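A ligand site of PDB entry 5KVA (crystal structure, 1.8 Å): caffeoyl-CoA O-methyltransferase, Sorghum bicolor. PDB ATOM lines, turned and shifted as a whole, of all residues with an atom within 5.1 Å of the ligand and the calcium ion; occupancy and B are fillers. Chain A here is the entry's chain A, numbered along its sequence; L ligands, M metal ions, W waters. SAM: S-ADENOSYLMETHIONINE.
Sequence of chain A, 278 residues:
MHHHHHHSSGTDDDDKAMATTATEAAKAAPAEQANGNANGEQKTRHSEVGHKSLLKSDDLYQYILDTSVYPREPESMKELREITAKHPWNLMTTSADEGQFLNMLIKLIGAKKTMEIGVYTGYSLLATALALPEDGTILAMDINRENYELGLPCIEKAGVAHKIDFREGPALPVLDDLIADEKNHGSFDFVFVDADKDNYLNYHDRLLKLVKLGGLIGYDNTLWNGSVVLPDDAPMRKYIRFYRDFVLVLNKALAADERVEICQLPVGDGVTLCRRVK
The calcium ion is bound by OD2 of Asp 220, OD1 of Asp 194, water W1, water W7, OD1 of Asn 221, water W3 and OD2 of Asp 194.
The calcium ion has seven donor atoms within binding distance.
The side-chain carboxylate of Asp 196 lies within hydrogen-bond range of the side-chain amide nitrogen of Asn 199.
The backbone carbonyl oxygen of Met 141 is in hydrogen-bond range of the backbone NH of Gly 118 (2.8 Å).
The side-chain carboxylate of Asp 142 is in hydrogen-bond range of the backbone NH of Val 119, at 2.7 Å.
O of Asp 142 sits at hydrogen-bond distance from N of Gly 169, 2.9 Å away.
O of Ile 117 lies within hydrogen-bond range of N of Asp 194 (2.8 Å).
The backbone NH (N) of Asn 144 sits at hydrogen-bond distance from the side-chain carboxylate (OD1) of Asp 142 (2.9 Å).
The side-chain hydroxyl (OH) of Tyr 203 sits at hydrogen-bond distance from the side-chain carboxylate (OD1) of Asp 196, at 2.7 Å.
OE2 of Glu 116 lies within hydrogen-bond range of N of Leu 125 (3.3 Å).
SD of Met 92 lies close to SD of the ligand, 3.8 Å away.
Residues that only touch the ligand: Val 119 (3.4 Å), Pro 170 (3.5 Å), Ala 195 (3.6 Å), Thr 93 (3.6 Å), Gly 169 (3.8 Å) and Tyr 123 (3.8 Å).
Within 4 Å of the ligand: Met 92, Thr 93, Thr 94, Glu 116, Gly 118, Val 119, Tyr 120, Tyr 123, Ser 124, Asp 142, Ile 143, Gly 169, Pro 170, Ala 171, Asp 194, Ala 195, Asp 196 and Tyr 203.
Water W7 lies within hydrogen-bond range of OG1 of Thr 94 (2.9 Å), O of Met 92 (3.0 Å) and O of Thr 93 (3.3 Å).
Water W4 lies within hydrogen-bond range of OXT of the ligand (2.6 Å), OG1 of Thr 93 (2.6 Å), OG1 of Thr 121 (2.8 Å), N of Tyr 123 (3.1 Å) and N of Gly 122 (3.5 Å).
Water W5 lies within hydrogen-bond range of OH of Tyr 203 (2.8 Å), N6 of the ligand (3.0 Å) and N of Ala 171 (3.3 Å).
Water W6 lies within hydrogen-bond range of OE1 of Glu 116, O of Val 119, OG of Ser 124, N of Leu 125, O of the ligand and N of Tyr 123.
The backbone NH (N) of Ser 124 sits at hydrogen-bond distance from an oxygen (O) of the ligand, 3.0 Å away.
A nitrogen (N1) of the ligand lies within hydrogen-bond range of the backbone NH (N) of Ala 171, 3.0 Å away.
An oxygen (O2') of the ligand is in hydrogen-bond range of the side-chain carboxylate of Asp 142, at 2.6 Å.
A nitrogen (N) of the ligand lies close to the side-chain carboxylate of Asp 194 (2.9 Å).
A nitrogen (N) of the ligand lies within hydrogen-bond range of the backbone carbonyl oxygen of Gly 118, 2.9 Å away.
OH of Tyr 203 lies within hydrogen-bond range of N6 of the ligand, at 3.3 Å.
O of the ligand lies close to N of Thr 94, 3.4 Å away.
The side-chain hydroxyl (OG) of Ser 124 sits at hydrogen-bond distance from a nitrogen (N) of the ligand (2.8 Å).
OE1 of Glu 116 is in salt-bridge range of N of the ligand (3.9 Å).
N of Tyr 120 sits at hydrogen-bond distance from O3' of the ligand, at 3.5 Å.
OD2 of Asp 196 is in hydrogen-bond range of N6 of the ligand (3.1 Å).
The side-chain hydroxyl (OG1) of Thr 94 is in hydrogen-bond range of an oxygen (O) of the ligand.
N of Ile 143 sits at hydrogen-bond distance from N3 of the ligand (3.5 Å).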
ATOM      1  N   MET A  92       2.237  28.868 -23.142  1.00  0.00           N
ATOM      2  CA  MET A  92       2.174  28.590 -21.716  1.00  0.00           C
ATOM      3  C   MET A  92       3.465  28.867 -20.961  1.00  0.00           C
ATOM      4  O   MET A  92       3.488  28.807 -19.738  1.00  0.00           O
ATOM      5  CB  MET A  92       1.790  27.125 -21.489  1.00  0.00           C
ATOM      6  CG  MET A  92       0.370  26.786 -21.857  1.00  0.00           C
ATOM      7  SD  MET A  92      -0.220  25.431 -20.838  1.00  0.00           S
ATOM      8  CE  MET A  92       0.991  24.164 -21.217  1.00  0.00           C
ATOM      9  N   THR A  93       4.547  29.132 -21.682  1.00  0.00           N
ATOM     10  CA  THR A  93       5.834  29.243 -21.005  1.00  0.00           C
ATOM     11  C   THR A  93       5.939  30.571 -20.244  1.00  0.00           C
ATOM     12  O   THR A  93       5.260  31.546 -20.553  1.00  0.00           O
ATOM     13  CB  THR A  93       7.037  29.127 -21.986  1.00  0.00           C
ATOM     14  OG1 THR A  93       8.234  28.939 -21.234  1.00  0.00           O
ATOM     15  CG2 THR A  93       7.169  30.367 -22.852  1.00  0.00           C
ATOM     16  N   THR A  94       6.771  30.599 -19.219  1.00  0.00           N
ATOM     17  CA  THR A  94       6.988  31.825 -18.463  1.00  0.00           C
ATOM     18  C   THR A  94       7.905  32.768 -19.255  1.00  0.00           C
ATOM     19  O   THR A  94       8.926  32.346 -19.791  1.00  0.00           O
ATOM     20  CB  THR A  94       7.587  31.500 -17.090  1.00  0.00           C
ATOM     21  OG1 THR A  94       6.631  30.715 -16.350  1.00  0.00           O
ATOM     22  CG2 THR A  94       7.939  32.762 -16.302  1.00  0.00           C
ATOM     23  N   GLU A 116       6.746  24.079  -6.915  1.00  0.00           N
ATOM     24  CA  GLU A 116       6.167  24.654  -8.124  1.00  0.00           C
ATOM     25  C   GLU A 116       4.997  23.785  -8.591  1.00  0.00           C
ATOM     26  O   GLU A 116       5.148  22.586  -8.790  1.00  0.00           O
ATOM     27  CB  GLU A 116       7.203  24.777  -9.255  1.00  0.00           C
ATOM     28  CG  GLU A 116       6.549  25.316 -10.533  1.00  0.00           C
ATOM     29  CD  GLU A 116       7.528  25.720 -11.609  1.00  0.00           C
ATOM     30  OE1 GLU A 116       7.575  25.019 -12.649  1.00  0.00           O
ATOM     31  OE2 GLU A 116       8.225  26.730 -11.433  1.00  0.00           O
ATOM     32  N   ILE A 117       3.828  24.418  -8.729  1.00  0.00           N
ATOM     33  CA  ILE A 117       2.642  23.760  -9.292  1.00  0.00           C
ATOM     34  C   ILE A 117       2.388  24.273 -10.719  1.00  0.00           C
ATOM     35  O   ILE A 117       2.031  25.433 -10.906  1.00  0.00           O
ATOM     36  CB  ILE A 117       1.406  24.001  -8.410  1.00  0.00           C
ATOM     37  CG1 ILE A 117       1.700  23.563  -6.962  1.00  0.00           C
ATOM     38  CG2 ILE A 117       0.201  23.274  -8.994  1.00  0.00           C
ATOM     39  CD1 ILE A 117       0.590  23.871  -5.964  1.00  0.00           C
ATOM     40  N   GLY A 118       2.597  23.414 -11.713  1.00  0.00           N
ATOM     41  CA  GLY A 118       2.466  23.828 -13.102  1.00  0.00           C
ATOM     42  C   GLY A 118       3.843  24.050 -13.696  1.00  0.00           C
ATOM     43  O   GLY A 118       4.401  25.136 -13.576  1.00  0.00           O
ATOM     44  N   VAL A 119       4.397  23.004 -14.311  1.00  0.00           N
ATOM     45  CA  VAL A 119       5.787  22.978 -14.744  1.00  0.00           C
ATOM     46  C   VAL A 119       5.970  23.157 -16.248  1.00  0.00           C
ATOM     47  O   VAL A 119       6.918  23.802 -16.689  1.00  0.00           O
ATOM     48  CB  VAL A 119       6.466  21.654 -14.342  1.00  0.00           C
ATOM     49  CG1 VAL A 119       7.918  21.625 -14.788  1.00  0.00           C
ATOM     50  CG2 VAL A 119       6.359  21.461 -12.830  1.00  0.00           C
ATOM     51  N   TYR A 120       5.080  22.556 -17.034  1.00  0.00           N
ATOM     52  CA  TYR A 120       5.195  22.568 -18.495  1.00  0.00           C
ATOM     53  C   TYR A 120       6.622  22.128 -18.881  1.00  0.00           C
ATOM     54  O   TYR A 120       7.089  21.094 -18.385  1.00  0.00           O
ATOM     55  CB  TYR A 120       4.803  23.955 -19.048  1.00  0.00           C
ATOM     56  CG  TYR A 120       4.847  24.071 -20.558  1.00  0.00           C
ATOM     57  CD1 TYR A 120       4.477  23.013 -21.380  1.00  0.00           C
ATOM     58  CD2 TYR A 120       5.283  25.255 -21.155  1.00  0.00           C
ATOM     59  CE1 TYR A 120       4.540  23.125 -22.769  1.00  0.00           C
ATOM     60  CE2 TYR A 120       5.358  25.372 -22.539  1.00  0.00           C
ATOM     61  CZ  TYR A 120       4.978  24.305 -23.341  1.00  0.00           C
ATOM     62  OH  TYR A 120       5.048  24.438 -24.706  1.00  0.00           O
ATOM     63  N   THR A 121       7.341  22.890 -19.708  1.00  0.00           N
ATOM     64  CA  THR A 121       8.686  22.475 -20.129  1.00  0.00           C
ATOM     65  C   THR A 121       9.803  22.950 -19.185  1.00  0.00           C
ATOM     66  O   THR A 121      10.955  22.575 -19.364  1.00  0.00           O
ATOM     67  CB  THR A 121       9.032  22.947 -21.549  1.00  0.00           C
ATOM     68  OG1 THR A 121       8.962  24.376 -21.625  1.00  0.00           O
ATOM     69  CG2 THR A 121       8.060  22.330 -22.563  1.00  0.00           C
ATOM     70  N   GLY A 122       9.456  23.777 -18.201  1.00  0.00           N
ATOM     71  CA  GLY A 122      10.376  24.045 -17.107  1.00  0.00           C
ATOM     72  C   GLY A 122      11.066  25.398 -16.995  1.00  0.00           C
ATOM     73  O   GLY A 122      11.986  25.522 -16.179  1.00  0.00           O
ATOM     74  N   TYR A 123      10.629  26.410 -17.728  1.00  0.00           N
ATOM     75  CA  TYR A 123      11.365  27.681 -17.695  1.00  0.00           C
ATOM     76  C   TYR A 123      11.351  28.305 -16.297  1.00  0.00           C
ATOM     77  O   TYR A 123      12.416  28.663 -15.784  1.00  0.00           O
ATOM     78  CB  TYR A 123      10.840  28.675 -18.734  1.00  0.00           C
ATOM     79  CG  TYR A 123      11.781  29.843 -18.990  1.00  0.00           C
ATOM     80  CD1 TYR A 123      12.872  29.716 -19.860  1.00  0.00           C
ATOM     81  CD2 TYR A 123      11.572  31.079 -18.383  1.00  0.00           C
ATOM     82  CE1 TYR A 123      13.732  30.783 -20.095  1.00  0.00           C
ATOM     83  CE2 TYR A 123      12.427  32.147 -18.605  1.00  0.00           C
ATOM     84  CZ  TYR A 123      13.503  31.995 -19.470  1.00  0.00           C
ATOM     85  OH  TYR A 123      14.334  33.077 -19.687  1.00  0.00           O
ATOM     86  N   SER A 124      10.185  28.439 -15.655  1.00  0.00           N
ATOM     87  CA  SER A 124      10.199  28.997 -14.298  1.00  0.00           C
ATOM     88  C   SER A 124      10.897  28.047 -13.329  1.00  0.00           C
ATOM     89  O   SER A 124      11.548  28.493 -12.384  1.00  0.00           O
ATOM     90  CB  SER A 124       8.777  29.315 -13.803  1.00  0.00           C
ATOM     91  OG  SER A 124       7.970  28.142 -13.708  1.00  0.00           O
ATOM     92  N   LEU A 125      10.787  26.747 -13.583  1.00  0.00           N
ATOM     93  CA  LEU A 125      11.417  25.766 -12.713  1.00  0.00           C
ATOM     94  C   LEU A 125      12.936  25.915 -12.761  1.00  0.00           C
ATOM     95  O   LEU A 125      13.600  25.896 -11.725  1.00  0.00           O
ATOM     96  CB  LEU A 125      11.025  24.342 -13.120  1.00  0.00           C
ATOM     97  CG  LEU A 125      11.502  23.238 -12.176  1.00  0.00           C
ATOM     98  CD1 LEU A 125      10.780  23.301 -10.828  1.00  0.00           C
ATOM     99  CD2 LEU A 125      11.303  21.861 -12.828  1.00  0.00           C
ATOM    100  N   MET A 141       5.233  19.849  -9.523  1.00  0.00           N
ATOM    101  CA  MET A 141       4.042  19.075  -9.859  1.00  0.00           C
ATOM    102  C   MET A 141       3.450  19.474 -11.209  1.00  0.00           C
ATOM    103  O   MET A 141       3.238  20.651 -11.489  1.00  0.00           O
ATOM    104  CB  MET A 141       2.974  19.235  -8.779  1.00  0.00           C
ATOM    105  CG  MET A 141       3.252  18.444  -7.511  1.00  0.00           C
ATOM    106  SD  MET A 141       2.416  19.147  -6.088  1.00  0.00           S
ATOM    107  CE  MET A 141       3.567  20.457  -5.710  1.00  0.00           C
ATOM    108  N   ASP A 142       3.170  18.471 -12.035  1.00  0.00           N
ATOM    109  CA  ASP A 142       2.389  18.682 -13.256  1.00  0.00           C
ATOM    110  C   ASP A 142       1.675  17.397 -13.645  1.00  0.00           C
ATOM    111  O   ASP A 142       2.200  16.298 -13.463  1.00  0.00           O
ATOM    112  CB  ASP A 142       3.279  19.141 -14.412  1.00  0.00           C
ATOM    113  CG  ASP A 142       2.533  19.969 -15.437  1.00  0.00           C
ATOM    114  OD1 ASP A 142       1.659  19.411 -16.132  1.00  0.00           O
ATOM    115  OD2 ASP A 142       2.801  21.187 -15.531  1.00  0.00           O
ATOM    116  N   ILE A 143       0.476  17.527 -14.207  1.00  0.00           N
ATOM    117  CA  ILE A 143      -0.251  16.363 -14.701  1.00  0.00           C
ATOM    118  C   ILE A 143       0.461  15.783 -15.914  1.00  0.00           C
ATOM    119  O   ILE A 143       0.308  14.612 -16.241  1.00  0.00           O
ATOM    120  CB  ILE A 143      -1.715  16.691 -15.070  1.00  0.00           C
ATOM    121  CG1 ILE A 143      -1.769  17.799 -16.127  1.00  0.00           C
ATOM    122  CG2 ILE A 143      -2.523  17.077 -13.837  1.00  0.00           C
ATOM    123  CD1 ILE A 143      -3.171  18.127 -16.617  1.00  0.00           C
ATOM    124  N   ASN A 144       1.259  16.617 -16.584  1.00  0.00           N
ATOM    125  CA  ASN A 144       1.931  16.239 -17.810  1.00  0.00           C
ATOM    126  C   ASN A 144       3.432  16.034 -17.603  1.00  0.00           C
ATOM    127  O   ASN A 144       4.171  16.988 -17.328  1.00  0.00           O
ATOM    128  CB  ASN A 144       1.662  17.296 -18.881  1.00  0.00           C
ATOM    129  CG  ASN A 144       2.162  16.881 -20.251  1.00  0.00           C
ATOM    130  OD1 ASN A 144       3.316  16.477 -20.418  1.00  0.00           O
ATOM    131  ND2 ASN A 144       1.285  17.007 -21.253  1.00  0.00           N
ATOM    132  N   GLY A 169       1.050  14.085 -12.053  1.00  0.00           N
ATOM    133  CA  GLY A 169      -0.313  13.973 -11.560  1.00  0.00           C
ATOM    134  C   GLY A 169      -0.861  15.287 -11.018  1.00  0.00           C
ATOM    135  O   GLY A 169      -0.133  16.281 -10.942  1.00  0.00           O
ATOM    136  N   PRO A 170      -2.150  15.291 -10.642  1.00  0.00           N
ATOM    137  CA  PRO A 170      -2.815  16.494 -10.107  1.00  0.00           C
ATOM    138  C   PRO A 170      -2.168  16.928  -8.803  1.00  0.00           C
ATOM    139  O   PRO A 170      -1.813  16.087  -7.980  1.00  0.00           O
ATOM    140  CB  PRO A 170      -4.254  16.019  -9.868  1.00  0.00           C
ATOM    141  CG  PRO A 170      -4.384  14.724 -10.597  1.00  0.00           C
ATOM    142  CD  PRO A 170      -3.029  14.115 -10.621  1.00  0.00           C
ATOM    143  N   ALA A 171      -2.004  18.229  -8.619  1.00  0.00           N
ATOM    144  CA  ALA A 171      -1.309  18.754  -7.447  1.00  0.00           C
ATOM    145  C   ALA A 171      -2.076  18.558  -6.142  1.00  0.00           C
ATOM    146  O   ALA A 171      -1.471  18.310  -5.098  1.00  0.00           O
ATOM    147  CB  ALA A 171      -0.999  20.242  -7.653  1.00  0.00           C
ATOM    148  N   PHE A 192       5.455  28.619  -6.180  1.00  0.00           N
ATOM    149  CA  PHE A 192       5.019  29.285  -7.407  1.00  0.00           C
ATOM    150  C   PHE A 192       3.869  28.470  -7.989  1.00  0.00           C
ATOM    151  O   PHE A 192       4.041  27.281  -8.296  1.00  0.00           O
ATOM    152  CB  PHE A 192       6.171  29.386  -8.414  1.00  0.00           C
ATOM    153  CG  PHE A 192       5.833  30.132  -9.683  1.00  0.00           C
ATOM    154  CD1 PHE A 192       5.327  31.422  -9.641  1.00  0.00           C
ATOM    155  CD2 PHE A 192       6.079  29.560 -10.923  1.00  0.00           C
ATOM    156  CE1 PHE A 192       5.064  32.125 -10.806  1.00  0.00           C
ATOM    157  CE2 PHE A 192       5.804  30.245 -12.099  1.00  0.00           C
ATOM    158  CZ  PHE A 192       5.284  31.535 -12.039  1.00  0.00           C
ATOM    159  N   ASP A 194       1.265  28.076 -10.919  1.00  0.00           N
ATOM    160  CA  ASP A 194       1.102  28.442 -12.321  1.00  0.00           C
ATOM    161  C   ASP A 194       0.384  27.316 -13.046  1.00  0.00           C
ATOM    162  O   ASP A 194       0.924  26.705 -13.985  1.00  0.00           O
ATOM    163  CB  ASP A 194       2.479  28.755 -12.942  1.00  0.00           C
ATOM    164  CG  ASP A 194       2.370  29.358 -14.318  1.00  0.00           C
ATOM    165  OD1 ASP A 194       1.270  29.796 -14.692  1.00  0.00           O
ATOM    166  OD2 ASP A 194       3.395  29.414 -15.040  1.00  0.00           O
ATOM    167  N   ALA A 195      -0.844  27.047 -12.625  1.00  0.00           N
ATOM    168  CA  ALA A 195      -1.563  25.878 -13.108  1.00  0.00           C
ATOM    169  C   ALA A 195      -3.013  26.197 -13.410  1.00  0.00           C
ATOM    170  O   ALA A 195      -3.304  27.158 -14.125  1.00  0.00           O
ATOM    171  CB  ALA A 195      -1.467  24.741 -12.093  1.00  0.00           C
ATOM    172  N   ASP A 196      -3.930  25.393 -12.866  1.00  0.00           N
ATOM    173  CA  ASP A 196      -5.344  25.543 -13.191  1.00  0.00           C
ATOM    174  C   ASP A 196      -6.027  26.561 -12.263  1.00  0.00           C
ATOM    175  O   ASP A 196      -6.178  26.311 -11.058  1.00  0.00           O
ATOM    176  CB  ASP A 196      -6.060  24.182 -13.136  1.00  0.00           C
ATOM    177  CG  ASP A 196      -5.705  23.347 -11.894  1.00  0.00           C
ATOM    178  OD1 ASP A 196      -4.631  23.555 -11.297  1.00  0.00           O
ATOM    179  OD2 ASP A 196      -6.506  22.470 -11.532  1.00  0.00           O
ATOM    180  N   ASN A 199      -8.636  26.161  -9.446  1.00  0.00           N
ATOM    181  CA  ASN A 199      -8.202  25.517  -8.215  1.00  0.00           C
ATOM    182  C   ASN A 199      -7.342  26.395  -7.302  1.00  0.00           C
ATOM    183  O   ASN A 199      -6.933  25.938  -6.236  1.00  0.00           O
ATOM    184  CB  ASN A 199      -7.433  24.215  -8.530  1.00  0.00           C
ATOM    185  CG  ASN A 199      -8.301  22.968  -8.342  1.00  0.00           C
ATOM    186  OD1 ASN A 199      -9.212  22.949  -7.520  1.00  0.00           O
ATOM    187  ND2 ASN A 199      -7.991  21.916  -9.095  1.00  0.00           N
ATOM    188  N   TYR A 203      -5.779  25.527  -3.646  1.00  0.00           N
ATOM    189  CA  TYR A 203      -4.340  25.450  -3.374  1.00  0.00           C
ATOM    190  C   TYR A 203      -3.968  26.371  -2.212  1.00  0.00           C
ATOM    191  O   TYR A 203      -3.214  25.984  -1.313  1.00  0.00           O
ATOM    192  CB  TYR A 203      -3.515  25.820  -4.604  1.00  0.00           C
ATOM    193  CG  TYR A 203      -3.672  24.869  -5.764  1.00  0.00           C
ATOM    194  CD1 TYR A 203      -3.907  23.518  -5.556  1.00  0.00           C
ATOM    195  CD2 TYR A 203      -3.589  25.328  -7.077  1.00  0.00           C
ATOM    196  CE1 TYR A 203      -4.054  22.640  -6.623  1.00  0.00           C
ATOM    197  CE2 TYR A 203      -3.731  24.461  -8.151  1.00  0.00           C
ATOM    198  CZ  TYR A 203      -3.955  23.122  -7.918  1.00  0.00           C
ATOM    199  OH  TYR A 203      -4.110  22.254  -8.974  1.00  0.00           O
ATOM    200  N   ASP A 220       0.395  32.899 -10.358  1.00  0.00           N
ATOM    201  CA  ASP A 220       0.715  33.397 -11.685  1.00  0.00           C
ATOM    202  C   ASP A 220      -0.521  33.700 -12.528  1.00  0.00           C
ATOM    203  O   ASP A 220      -1.575  33.102 -12.332  1.00  0.00           O
ATOM    204  CB  ASP A 220       1.594  32.403 -12.426  1.00  0.00           C
ATOM    205  CG  ASP A 220       2.630  33.102 -13.269  1.00  0.00           C
ATOM    206  OD1 ASP A 220       3.031  34.212 -12.893  1.00  0.00           O
ATOM    207  OD2 ASP A 220       3.045  32.529 -14.299  1.00  0.00           O
ATOM    208  N   ASN A 221      -0.353  34.639 -13.454  1.00  0.00           N
ATOM    209  CA  ASN A 221      -1.363  35.028 -14.444  1.00  0.00           C
ATOM    210  C   ASN A 221      -2.591  35.713 -13.839  1.00  0.00           C
ATOM    211  O   ASN A 221      -3.675  35.601 -14.392  1.00  0.00           O
ATOM    212  CB  ASN A 221      -1.839  33.816 -15.247  1.00  0.00           C
ATOM    213  CG  ASN A 221      -0.717  33.197 -16.069  1.00  0.00           C
ATOM    214  OD1 ASN A 221       0.076  32.436 -15.539  1.00  0.00           O
ATOM    215  ND2 ASN A 221      -0.647  33.560 -17.359  1.00  0.00           N
HETATM  216  N   SAM L   1       5.532  27.405 -14.955  1.00  0.00           N
HETATM  217  CA  SAM L   1       5.504  26.835 -16.300  1.00  0.00           C
HETATM  218  C   SAM L   1       6.586  27.364 -17.217  1.00  0.00           C
HETATM  219  O   SAM L   1       7.390  28.235 -16.851  1.00  0.00           O
HETATM  220  OXT SAM L   1       6.693  26.922 -18.360  1.00  0.00           O
HETATM  221  CB  SAM L   1       4.155  27.041 -16.983  1.00  0.00           C
HETATM  222  CG  SAM L   1       3.040  26.155 -16.435  1.00  0.00           C
HETATM  223  SD  SAM L   1       1.660  26.103 -17.613  1.00  0.00           S
HETATM  224  CE  SAM L   1       1.113  27.828 -17.531  1.00  0.00           C
HETATM  225  C5' SAM L   1       0.334  25.293 -16.668  1.00  0.00           C
HETATM  226  C4' SAM L   1       0.673  23.850 -16.327  1.00  0.00           C
HETATM  227  O4' SAM L   1      -0.157  23.371 -15.282  1.00  0.00           O
HETATM  228  C3' SAM L   1       0.454  22.912 -17.512  1.00  0.00           C
HETATM  229  O3' SAM L   1       1.694  22.309 -17.840  1.00  0.00           O
HETATM  230  C2' SAM L   1      -0.559  21.881 -17.027  1.00  0.00           C
HETATM  231  O2' SAM L   1      -0.229  20.563 -17.416  1.00  0.00           O
HETATM  232  C1' SAM L   1      -0.455  22.016 -15.525  1.00  0.00           C
HETATM  233  N9  SAM L   1      -1.683  21.694 -14.776  1.00  0.00           N
HETATM  234  C8  SAM L   1      -2.992  21.993 -15.059  1.00  0.00           C
HETATM  235  N7  SAM L   1      -3.762  21.503 -14.059  1.00  0.00           N
HETATM  236  C5  SAM L   1      -2.955  20.919 -13.143  1.00  0.00           C
HETATM  237  C6  SAM L   1      -3.183  20.275 -11.945  1.00  0.00           C
HETATM  238  N6  SAM L   1      -4.420  20.129 -11.468  1.00  0.00           N
HETATM  239  N1  SAM L   1      -2.114  19.768 -11.222  1.00  0.00           N
HETATM  240  C2  SAM L   1      -0.826  19.890 -11.699  1.00  0.00           C
HETATM  241  N3  SAM L   1      -0.597  20.546 -12.891  1.00  0.00           N
HETATM  242  C4  SAM L   1      -1.640  21.036 -13.594  1.00  0.00           C
HETATM  243 CA    CA M   1       2.204  31.391 -16.139  1.00  0.00          CA
HETATM  244  O   HOH W   1       1.037  30.949 -18.129  1.00  0.00           O
HETATM  245  O   HOH W   2       2.726  20.415 -19.569  1.00  0.00           O
HETATM  246  O   HOH W   3       2.605  33.656 -17.156  1.00  0.00           O
HETATM  247  O   HOH W   4       8.649  26.613 -20.049  1.00  0.00           O
HETATM  248  O   HOH W   5      -4.999  19.576  -8.599  1.00  0.00           O
HETATM  249  O   HOH W   6       8.458  25.593 -15.129  1.00  0.00           O
HETATM  250  O   HOH W   7       4.032  30.793 -17.624  1.00  0.00           O
HETATM  251  O   HOH W   8      -1.682  19.533 -19.520  1.00  0.00           O
HETATM  252  O   HOH W   9      -6.154  20.651 -14.829  1.00  0.00           O
